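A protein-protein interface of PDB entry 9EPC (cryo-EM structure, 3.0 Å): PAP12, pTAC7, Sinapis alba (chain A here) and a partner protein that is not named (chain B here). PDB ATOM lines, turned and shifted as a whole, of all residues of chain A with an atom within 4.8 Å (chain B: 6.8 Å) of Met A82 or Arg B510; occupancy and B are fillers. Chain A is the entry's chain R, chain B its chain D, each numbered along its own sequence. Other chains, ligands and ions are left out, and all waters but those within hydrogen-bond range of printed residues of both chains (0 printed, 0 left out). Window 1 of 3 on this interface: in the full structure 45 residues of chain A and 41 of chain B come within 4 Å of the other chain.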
ATOM      1  N   GLY A  79     -17.068   1.559   8.111  1.00  0.00           N
ATOM      2  CA  GLY A  79     -18.011   0.738   7.386  1.00  0.00           C
ATOM      3  C   GLY A  79     -19.467   1.022   7.673  1.00  0.00           C
ATOM      4  O   GLY A  79     -20.324   0.231   7.265  1.00  0.00           O
ATOM      5  N   LYS A  80     -19.778   2.119   8.364  1.00  0.00           N
ATOM      6  CA  LYS A  80     -21.166   2.454   8.651  1.00  0.00           C
ATOM      7  C   LYS A  80     -21.932   2.900   7.416  1.00  0.00           C
ATOM      8  O   LYS A  80     -23.163   2.987   7.475  1.00  0.00           O
ATOM      9  CB  LYS A  80     -21.235   3.547   9.715  1.00  0.00           C
ATOM     10  CG  LYS A  80     -20.622   3.159  11.044  1.00  0.00           C
ATOM     11  CD  LYS A  80     -20.735   4.293  12.044  1.00  0.00           C
ATOM     12  CE  LYS A  80     -20.100   3.917  13.367  1.00  0.00           C
ATOM     13  NZ  LYS A  80     -20.180   5.028  14.354  1.00  0.00           N
ATOM     14  N   VAL A  81     -21.246   3.196   6.311  1.00  0.00           N
ATOM     15  CA  VAL A  81     -21.949   3.590   5.096  1.00  0.00           C
ATOM     16  C   VAL A  81     -22.782   2.432   4.566  1.00  0.00           C
ATOM     17  O   VAL A  81     -23.891   2.629   4.057  1.00  0.00           O
ATOM     18  CB  VAL A  81     -20.953   4.118   4.046  1.00  0.00           C
ATOM     19  CG1 VAL A  81     -19.835   3.114   3.813  1.00  0.00           C
ATOM     20  CG2 VAL A  81     -21.670   4.444   2.748  1.00  0.00           C
ATOM     21  N   MET A  82     -22.273   1.204   4.689  1.00  0.00           N
ATOM     22  CA  MET A  82     -23.070   0.041   4.323  1.00  0.00           C
ATOM     23  C   MET A  82     -24.249  -0.146   5.265  1.00  0.00           C
ATOM     24  O   MET A  82     -25.313  -0.606   4.840  1.00  0.00           O
ATOM     25  CB  MET A  82     -22.204  -1.215   4.315  1.00  0.00           C
ATOM     26  CG  MET A  82     -22.995  -2.504   4.163  1.00  0.00           C
ATOM     27  SD  MET A  82     -21.963  -3.977   4.092  1.00  0.00           S
ATOM     28  CE  MET A  82     -20.510  -3.410   4.967  1.00  0.00           C
ATOM     29  N   THR A  83     -24.078   0.207   6.542  1.00  0.00           N
ATOM     30  CA  THR A  83     -25.154   0.048   7.514  1.00  0.00           C
ATOM     31  C   THR A  83     -26.392   0.830   7.094  1.00  0.00           C
ATOM     32  O   THR A  83     -27.516   0.321   7.160  1.00  0.00           O
ATOM     33  CB  THR A  83     -24.672   0.493   8.895  1.00  0.00           C
ATOM     34  OG1 THR A  83     -23.864  -0.538   9.478  1.00  0.00           O
ATOM     35  CG2 THR A  83     -25.847   0.798   9.807  1.00  0.00           C
ATOM     36  N   MET A  84     -26.202   2.073   6.651  1.00  0.00           N
ATOM     37  CA  MET A  84     -27.323   2.839   6.124  1.00  0.00           C
ATOM     38  C   MET A  84     -27.875   2.201   4.857  1.00  0.00           C
ATOM     39  O   MET A  84     -29.094   2.168   4.651  1.00  0.00           O
ATOM     40  CB  MET A  84     -26.893   4.279   5.856  1.00  0.00           C
ATOM     41  CG  MET A  84     -27.960   5.156   5.218  1.00  0.00           C
ATOM     42  SD  MET A  84     -29.042   5.983   6.401  1.00  0.00           S
ATOM     43  CE  MET A  84     -30.297   4.738   6.680  1.00  0.00           C
ATOM     44  N   ASP A  85     -26.993   1.691   3.997  1.00  0.00           N
ATOM     45  CA  ASP A  85     -27.444   1.038   2.774  1.00  0.00           C
ATOM     46  C   ASP A  85     -28.217  -0.237   3.081  1.00  0.00           C
ATOM     47  O   ASP A  85     -29.199  -0.553   2.399  1.00  0.00           O
ATOM     48  CB  ASP A  85     -26.251   0.738   1.870  1.00  0.00           C
ATOM     49  CG  ASP A  85     -25.532   1.991   1.426  1.00  0.00           C
ATOM     50  OD1 ASP A  85     -26.180   3.057   1.368  1.00  0.00           O
ATOM     51  OD2 ASP A  85     -24.322   1.913   1.132  1.00  0.00           O
ATOM     52  N   ILE A  86     -27.787  -0.984   4.098  1.00  0.00           N
ATOM     53  CA  ILE A  86     -28.500  -2.199   4.484  1.00  0.00           C
ATOM     54  C   ILE A  86     -29.922  -1.863   4.913  1.00  0.00           C
ATOM     55  O   ILE A  86     -30.883  -2.533   4.518  1.00  0.00           O
ATOM     56  CB  ILE A  86     -27.736  -2.938   5.596  1.00  0.00           C
ATOM     57  CG1 ILE A  86     -26.475  -3.591   5.031  1.00  0.00           C
ATOM     58  CG2 ILE A  86     -28.629  -3.966   6.262  1.00  0.00           C
ATOM     59  CD1 ILE A  86     -25.596  -4.213   6.083  1.00  0.00           C
ATOM     60  N   PHE A 126     -20.873  -8.646   0.482  1.00  0.00           N
ATOM     61  CA  PHE A 126     -20.735  -7.203   0.319  1.00  0.00           C
ATOM     62  C   PHE A 126     -20.908  -6.796  -1.136  1.00  0.00           C
ATOM     63  O   PHE A 126     -21.449  -5.724  -1.428  1.00  0.00           O
ATOM     64  CB  PHE A 126     -19.380  -6.732   0.845  1.00  0.00           C
ATOM     65  CG  PHE A 126     -19.294  -6.674   2.342  1.00  0.00           C
ATOM     66  CD1 PHE A 126     -20.261  -7.263   3.135  1.00  0.00           C
ATOM     67  CD2 PHE A 126     -18.246  -6.014   2.956  1.00  0.00           C
ATOM     68  CE1 PHE A 126     -20.179  -7.207   4.508  1.00  0.00           C
ATOM     69  CE2 PHE A 126     -18.162  -5.951   4.329  1.00  0.00           C
ATOM     70  CZ  PHE A 126     -19.129  -6.550   5.106  1.00  0.00           C
ATOM     71  N   LEU A 129     -24.599  -6.546  -1.757  1.00  0.00           N
ATOM     72  CA  LEU A 129     -25.176  -5.337  -1.179  1.00  0.00           C
ATOM     73  C   LEU A 129     -24.798  -4.103  -1.987  1.00  0.00           C
ATOM     74  O   LEU A 129     -25.634  -3.222  -2.214  1.00  0.00           O
ATOM     75  CB  LEU A 129     -24.733  -5.191   0.274  1.00  0.00           C
ATOM     76  CG  LEU A 129     -25.179  -6.323   1.200  1.00  0.00           C
ATOM     77  CD1 LEU A 129     -24.665  -6.104   2.611  1.00  0.00           C
ATOM     78  CD2 LEU A 129     -26.691  -6.446   1.192  1.00  0.00           C
ATOM     79  N   TYR A 144     -17.946  -2.482  -1.252  1.00  0.00           N
ATOM     80  CA  TYR A 144     -17.523  -1.553  -0.206  1.00  0.00           C
ATOM     81  C   TYR A 144     -16.058  -1.729   0.171  1.00  0.00           C
ATOM     82  O   TYR A 144     -15.652  -1.366   1.279  1.00  0.00           O
ATOM     83  CB  TYR A 144     -18.402  -1.683   1.043  1.00  0.00           C
ATOM     84  CG  TYR A 144     -19.860  -1.383   0.802  1.00  0.00           C
ATOM     85  CD1 TYR A 144     -20.340  -0.084   0.855  1.00  0.00           C
ATOM     86  CD2 TYR A 144     -20.760  -2.401   0.530  1.00  0.00           C
ATOM     87  CE1 TYR A 144     -21.672   0.193   0.638  1.00  0.00           C
ATOM     88  CE2 TYR A 144     -22.094  -2.134   0.313  1.00  0.00           C
ATOM     89  CZ  TYR A 144     -22.543  -0.836   0.368  1.00  0.00           C
ATOM     90  OH  TYR A 144     -23.872  -0.565   0.151  1.00  0.00           O
ATOM     91  N   HIS B 393     -20.474  -1.471  16.371  1.00  0.00           N
ATOM     92  CA  HIS B 393     -20.620  -2.757  15.703  1.00  0.00           C
ATOM     93  C   HIS B 393     -19.299  -3.492  15.524  1.00  0.00           C
ATOM     94  O   HIS B 393     -19.255  -4.492  14.801  1.00  0.00           O
ATOM     95  CB  HIS B 393     -21.292  -2.561  14.344  1.00  0.00           C
ATOM     96  CG  HIS B 393     -20.513  -1.690  13.412  1.00  0.00           C
ATOM     97  ND1 HIS B 393     -19.396  -2.133  12.738  1.00  0.00           N
ATOM     98  CD2 HIS B 393     -20.686  -0.398  13.046  1.00  0.00           C
ATOM     99  CE1 HIS B 393     -18.916  -1.153  11.993  1.00  0.00           C
ATOM    100  NE2 HIS B 393     -19.682  -0.089  12.162  1.00  0.00           N
ATOM    101  N   GLY B 447     -14.845  -7.806   6.607  1.00  0.00           N
ATOM    102  CA  GLY B 447     -16.139  -8.132   6.053  1.00  0.00           C
ATOM    103  C   GLY B 447     -16.735  -9.440   6.517  1.00  0.00           C
ATOM    104  O   GLY B 447     -17.837  -9.787   6.077  1.00  0.00           O
ATOM    105  N   PRO B 449     -18.271 -11.221   9.629  1.00  0.00           N
ATOM    106  CA  PRO B 449     -18.700 -11.031  11.016  1.00  0.00           C
ATOM    107  C   PRO B 449     -18.488 -12.284  11.852  1.00  0.00           C
ATOM    108  O   PRO B 449     -18.433 -13.406  11.346  1.00  0.00           O
ATOM    109  CB  PRO B 449     -20.190 -10.705  10.879  1.00  0.00           C
ATOM    110  CG  PRO B 449     -20.593 -11.399   9.630  1.00  0.00           C
ATOM    111  CD  PRO B 449     -19.414 -11.301   8.704  1.00  0.00           C
ATOM    112  N   SER B 465     -23.462 -10.256  17.002  1.00  0.00           N
ATOM    113  CA  SER B 465     -22.476 -10.276  15.933  1.00  0.00           C
ATOM    114  C   SER B 465     -21.782  -8.927  15.820  1.00  0.00           C
ATOM    115  O   SER B 465     -22.428  -7.876  15.876  1.00  0.00           O
ATOM    116  CB  SER B 465     -23.120 -10.636  14.595  1.00  0.00           C
ATOM    117  OG  SER B 465     -24.028  -9.634  14.189  1.00  0.00           O
ATOM    118  N   GLN B 467     -18.242  -6.913  13.709  1.00  0.00           N
ATOM    119  CA  GLN B 467     -17.216  -6.985  12.683  1.00  0.00           C
ATOM    120  C   GLN B 467     -15.859  -7.005  13.368  1.00  0.00           C
ATOM    121  O   GLN B 467     -15.476  -6.001  13.987  1.00  0.00           O
ATOM    122  CB  GLN B 467     -17.316  -5.803  11.733  1.00  0.00           C
ATOM    123  CG  GLN B 467     -16.118  -5.649  10.819  1.00  0.00           C
ATOM    124  CD  GLN B 467     -15.824  -6.905  10.028  1.00  0.00           C
ATOM    125  OE1 GLN B 467     -16.735  -7.577   9.549  1.00  0.00           O
ATOM    126  NE2 GLN B 467     -14.546  -7.232   9.893  1.00  0.00           N
ATOM    127  N   ALA B 505     -25.091 -18.219   6.651  1.00  0.00           N
ATOM    128  CA  ALA B 505     -24.869 -17.814   8.035  1.00  0.00           C
ATOM    129  C   ALA B 505     -24.202 -16.449   8.111  1.00  0.00           C
ATOM    130  O   ALA B 505     -24.579 -15.614   8.941  1.00  0.00           O
ATOM    131  CB  ALA B 505     -24.030 -18.862   8.761  1.00  0.00           C
ATOM    132  N   GLN B 506     -23.208 -16.203   7.254  1.00  0.00           N
ATOM    133  CA  GLN B 506     -22.565 -14.896   7.233  1.00  0.00           C
ATOM    134  C   GLN B 506     -23.537 -13.807   6.808  1.00  0.00           C
ATOM    135  O   GLN B 506     -23.406 -12.656   7.239  1.00  0.00           O
ATOM    136  CB  GLN B 506     -21.358 -14.916   6.298  1.00  0.00           C
ATOM    137  CG  GLN B 506     -20.327 -15.974   6.622  1.00  0.00           C
ATOM    138  CD  GLN B 506     -19.179 -15.973   5.636  1.00  0.00           C
ATOM    139  OE1 GLN B 506     -18.962 -14.997   4.920  1.00  0.00           O
ATOM    140  NE2 GLN B 506     -18.441 -17.076   5.587  1.00  0.00           N
ATOM    141  N   ALA B 507     -24.509 -14.146   5.962  1.00  0.00           N
ATOM    142  CA  ALA B 507     -25.495 -13.160   5.537  1.00  0.00           C
ATOM    143  C   ALA B 507     -26.376 -12.727   6.701  1.00  0.00           C
ATOM    144  O   ALA B 507     -26.549 -11.529   6.949  1.00  0.00           O
ATOM    145  CB  ALA B 507     -26.345 -13.724   4.400  1.00  0.00           C
ATOM    146  N   GLU B 508     -26.934 -13.687   7.436  1.00  0.00           N
ATOM    147  CA  GLU B 508     -27.843 -13.337   8.519  1.00  0.00           C
ATOM    148  C   GLU B 508     -27.106 -12.802   9.739  1.00  0.00           C
ATOM    149  O   GLU B 508     -27.690 -12.048  10.524  1.00  0.00           O
ATOM    150  CB  GLU B 508     -28.703 -14.542   8.893  1.00  0.00           C
ATOM    151  CG  GLU B 508     -27.930 -15.799   9.208  1.00  0.00           C
ATOM    152  CD  GLU B 508     -28.833 -17.008   9.315  1.00  0.00           C
ATOM    153  OE1 GLU B 508     -29.893 -17.015   8.657  1.00  0.00           O
ATOM    154  OE2 GLU B 508     -28.491 -17.947  10.059  1.00  0.00           O
ATOM    155  N   ALA B 509     -25.840 -13.177   9.921  1.00  0.00           N
ATOM    156  CA  ALA B 509     -25.049 -12.568  10.983  1.00  0.00           C
ATOM    157  C   ALA B 509     -24.871 -11.077  10.742  1.00  0.00           C
ATOM    158  O   ALA B 509     -24.981 -10.270  11.671  1.00  0.00           O
ATOM    159  CB  ALA B 509     -23.691 -13.259  11.090  1.00  0.00           C
ATOM    160  N   ARG B 510     -24.599 -10.693   9.496  1.00  0.00           N
ATOM    161  CA  ARG B 510     -24.393  -9.291   9.162  1.00  0.00           C
ATOM    162  C   ARG B 510     -25.700  -8.515   9.082  1.00  0.00           C
ATOM    163  O   ARG B 510     -25.725  -7.319   9.392  1.00  0.00           O
ATOM    164  CB  ARG B 510     -23.638  -9.182   7.836  1.00  0.00           C
ATOM    165  CG  ARG B 510     -23.278  -7.770   7.428  1.00  0.00           C
ATOM    166  CD  ARG B 510     -22.340  -7.135   8.433  1.00  0.00           C
ATOM    167  NE  ARG B 510     -22.041  -5.749   8.096  1.00  0.00           N
ATOM    168  CZ  ARG B 510     -22.819  -4.723   8.409  1.00  0.00           C
ATOM    169  NH1 ARG B 510     -23.959  -4.891   9.057  1.00  0.00           N
ATOM    170  NH2 ARG B 510     -22.444  -3.495   8.058  1.00  0.00           N
ATOM    171  N   LEU B 511     -26.790  -9.168   8.680  1.00  0.00           N
ATOM    172  CA  LEU B 511     -28.034  -8.477   8.379  1.00  0.00           C
ATOM    173  C   LEU B 511     -29.111  -8.627   9.444  1.00  0.00           C
ATOM    174  O   LEU B 511     -30.151  -7.970   9.335  1.00  0.00           O
ATOM    175  CB  LEU B 511     -28.598  -8.966   7.038  1.00  0.00           C
ATOM    176  CG  LEU B 511     -27.700  -8.793   5.813  1.00  0.00           C
ATOM    177  CD1 LEU B 511     -28.318  -9.464   4.603  1.00  0.00           C
ATOM    178  CD2 LEU B 511     -27.454  -7.327   5.539  1.00  0.00           C
ATOM    179  N   LEU B 512     -28.907  -9.460  10.462  1.00  0.00           N
ATOM    180  CA  LEU B 512     -29.957  -9.659  11.454  1.00  0.00           C
ATOM    181  C   LEU B 512     -29.454  -9.487  12.880  1.00  0.00           C
ATOM    182  O   LEU B 512     -30.203  -9.043  13.756  1.00  0.00           O
ATOM    183  CB  LEU B 512     -30.582 -11.045  11.294  1.00  0.00           C
ATOM    184  CG  LEU B 512     -31.328 -11.308   9.987  1.00  0.00           C
ATOM    185  CD1 LEU B 512     -31.853 -12.729   9.956  1.00  0.00           C
ATOM    186  CD2 LEU B 512     -32.462 -10.315   9.819  1.00  0.00           C
ATOM    187  N   MET B 513     -28.192  -9.830  13.131  1.00  0.00           N
ATOM    188  CA  MET B 513     -27.658  -9.848  14.483  1.00  0.00           C
ATOM    189  C   MET B 513     -26.734  -8.680  14.792  1.00  0.00           C
ATOM    190  O   MET B 513     -26.231  -8.595  15.916  1.00  0.00           O
ATOM    191  CB  MET B 513     -26.915 -11.164  14.738  1.00  0.00           C
ATOM    192  CG  MET B 513     -27.793 -12.394  14.677  1.00  0.00           C
ATOM    193  SD  MET B 513     -26.910 -13.874  15.194  1.00  0.00           S
ATOM    194  CE  MET B 513     -26.508 -13.441  16.884  1.00  0.00           C
ATOM    195  N   PHE B 514     -26.488  -7.789  13.840  1.00  0.00           N
ATOM    196  CA  PHE B 514     -25.584  -6.678  14.097  1.00  0.00           C
ATOM    197  C   PHE B 514     -26.217  -5.680  15.059  1.00  0.00           C
ATOM    198  O   PHE B 514     -27.438  -5.522  15.116  1.00  0.00           O
ATOM    199  CB  PHE B 514     -25.194  -5.989  12.793  1.00  0.00           C
ATOM    200  CG  PHE B 514     -23.766  -6.215  12.399  1.00  0.00           C
ATOM    201  CD1 PHE B 514     -23.391  -7.379  11.756  1.00  0.00           C
ATOM    202  CD2 PHE B 514     -22.801  -5.265  12.669  1.00  0.00           C
ATOM    203  CE1 PHE B 514     -22.080  -7.594  11.395  1.00  0.00           C
ATOM    204  CE2 PHE B 514     -21.488  -5.476  12.307  1.00  0.00           C
ATOM    205  CZ  PHE B 514     -21.128  -6.642  11.669  1.00  0.00           C
ATOM    206  N   HIS B 516     -26.300  -2.484  15.115  1.00  0.00           N
ATOM    207  CA  HIS B 516     -26.950  -1.300  14.571  1.00  0.00           C
ATOM    208  C   HIS B 516     -28.394  -1.547  14.160  1.00  0.00           C
ATOM    209  O   HIS B 516     -29.108  -0.583  13.869  1.00  0.00           O
ATOM    210  CB  HIS B 516     -26.158  -0.766  13.376  1.00  0.00           C
ATOM    211  CG  HIS B 516     -26.150  -1.684  12.194  1.00  0.00           C
ATOM    212  ND1 HIS B 516     -27.204  -1.768  11.309  1.00  0.00           N
ATOM    213  CD2 HIS B 516     -25.212  -2.549  11.744  1.00  0.00           C
ATOM    214  CE1 HIS B 516     -26.915  -2.647  10.366  1.00  0.00           C
ATOM    215  NE2 HIS B 516     -25.713  -3.137  10.608  1.00  0.00           N
ATOM    216  N   MET B 517     -28.839  -2.803  14.121  1.00  0.00           N
ATOM    217  CA  MET B 517     -30.223  -3.124  13.809  1.00  0.00           C
ATOM    218  C   MET B 517     -31.010  -3.629  15.007  1.00  0.00           C
ATOM    219  O   MET B 517     -32.217  -3.857  14.881  1.00  0.00           O
ATOM    220  CB  MET B 517     -30.291  -4.169  12.689  1.00  0.00           C
ATOM    221  CG  MET B 517     -30.021  -3.605  11.311  1.00  0.00           C
ATOM    222  SD  MET B 517     -29.662  -4.899  10.118  1.00  0.00           S
ATOM    223  CE  MET B 517     -28.309  -5.723  10.949  1.00  0.00           C
ATOM    224  N   CYS B 676     -23.293   8.926   3.580  1.00  0.00           N
ATOM    225  CA  CYS B 676     -24.273   8.167   2.808  1.00  0.00           C
ATOM    226  C   CYS B 676     -24.957   9.081   1.791  1.00  0.00           C
ATOM    227  O   CYS B 676     -26.170   9.285   1.795  1.00  0.00           O
ATOM    228  CB  CYS B 676     -25.281   7.514   3.743  1.00  0.00           C
ATOM    229  SG  CYS B 676     -24.519   6.745   5.186  1.00  0.00           S
ATOM    230  N   TYR B 678     -26.695   9.842  -0.878  1.00  0.00           N
ATOM    231  CA  TYR B 678     -27.605   9.345  -1.902  1.00  0.00           C
ATOM    232  C   TYR B 678     -27.922  10.402  -2.951  1.00  0.00           C
ATOM    233  O   TYR B 678     -28.401  10.056  -4.035  1.00  0.00           O
ATOM    234  CB  TYR B 678     -28.900   8.846  -1.261  1.00  0.00           C
ATOM    235  CG  TYR B 678     -28.778   7.476  -0.637  1.00  0.00           C
ATOM    236  CD1 TYR B 678     -28.024   6.482  -1.244  1.00  0.00           C
ATOM    237  CD2 TYR B 678     -29.411   7.180   0.562  1.00  0.00           C
ATOM    238  CE1 TYR B 678     -27.909   5.230  -0.678  1.00  0.00           C
ATOM    239  CE2 TYR B 678     -29.299   5.930   1.136  1.00  0.00           C
ATOM    240  CZ  TYR B 678     -28.547   4.959   0.511  1.00  0.00           C
ATOM    241  OH  TYR B 678     -28.432   3.713   1.079  1.00  0.00           O
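His B393 touches Lys A80.
Met A82 touches Arg B510.
Arg B510 touches Thr A83.
Met A84 touches Cys B676.
Met A84 touches Tyr B678.
Ile A86 touches Arg B510 (CD1 to NH1, 3.5 Å).
CD2 of Leu B511 touches CG2 of Ile A86 (3.6 Å).
CE2 of Phe A126 touches CA of Gly B447, at 3.4 Å.
The side-chain hydroxyl (OH) of Tyr A144 is in hydrogen-bond range of the side-chain carboxylate (OD2) of Asp A85, 2.7 Å away.
The backbone carbonyl oxygen (O) of His B393 sits at hydrogen-bond distance from the backbone NH (N) of Gln B467, 2.8 Å away.
The backbone NH (N) of Gly B447 lies close to the side-chain amide nitrogen (NE2) of Gln B467 (3.3 Å).
The guanidinium group (NH1) of Arg B510 is in hydrogen-bond range of a ring nitrogen (NE2) of His B516 (2.9 Å).
Printed residues of chain B within 4 Å of Lys A80: His B393.
Printed residues of chain B within 4 Å of Met A82: Arg B510.
Of the printed residues of chain B, Thr A83 touches Arg B510 and His B516.
Gln B506 touches none of the printed residues of chain A.
Of the printed residues of chain A, Cys B676 touches Met A84 (3.5 Å).
Printed residues of chain A within 4 Å of Tyr B678: Met A84 and Asp A85.
Of the 19 printed residues of chain B, 7 touch a printed residue of chain A.
Hydrophobic or aromatic side chains of chain A within 4 Å of the printed part of chain B: Met A82, Met A84, Ile A86 and Phe A126.
Among the printed residues, 10 pairs touch across the chains.
OG1 of Thr A83 sits close to NE2 of His B516, 3.4 Å away.
OD1 of Asp A85 lies close to OH of Tyr B678 (2.4 Å).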
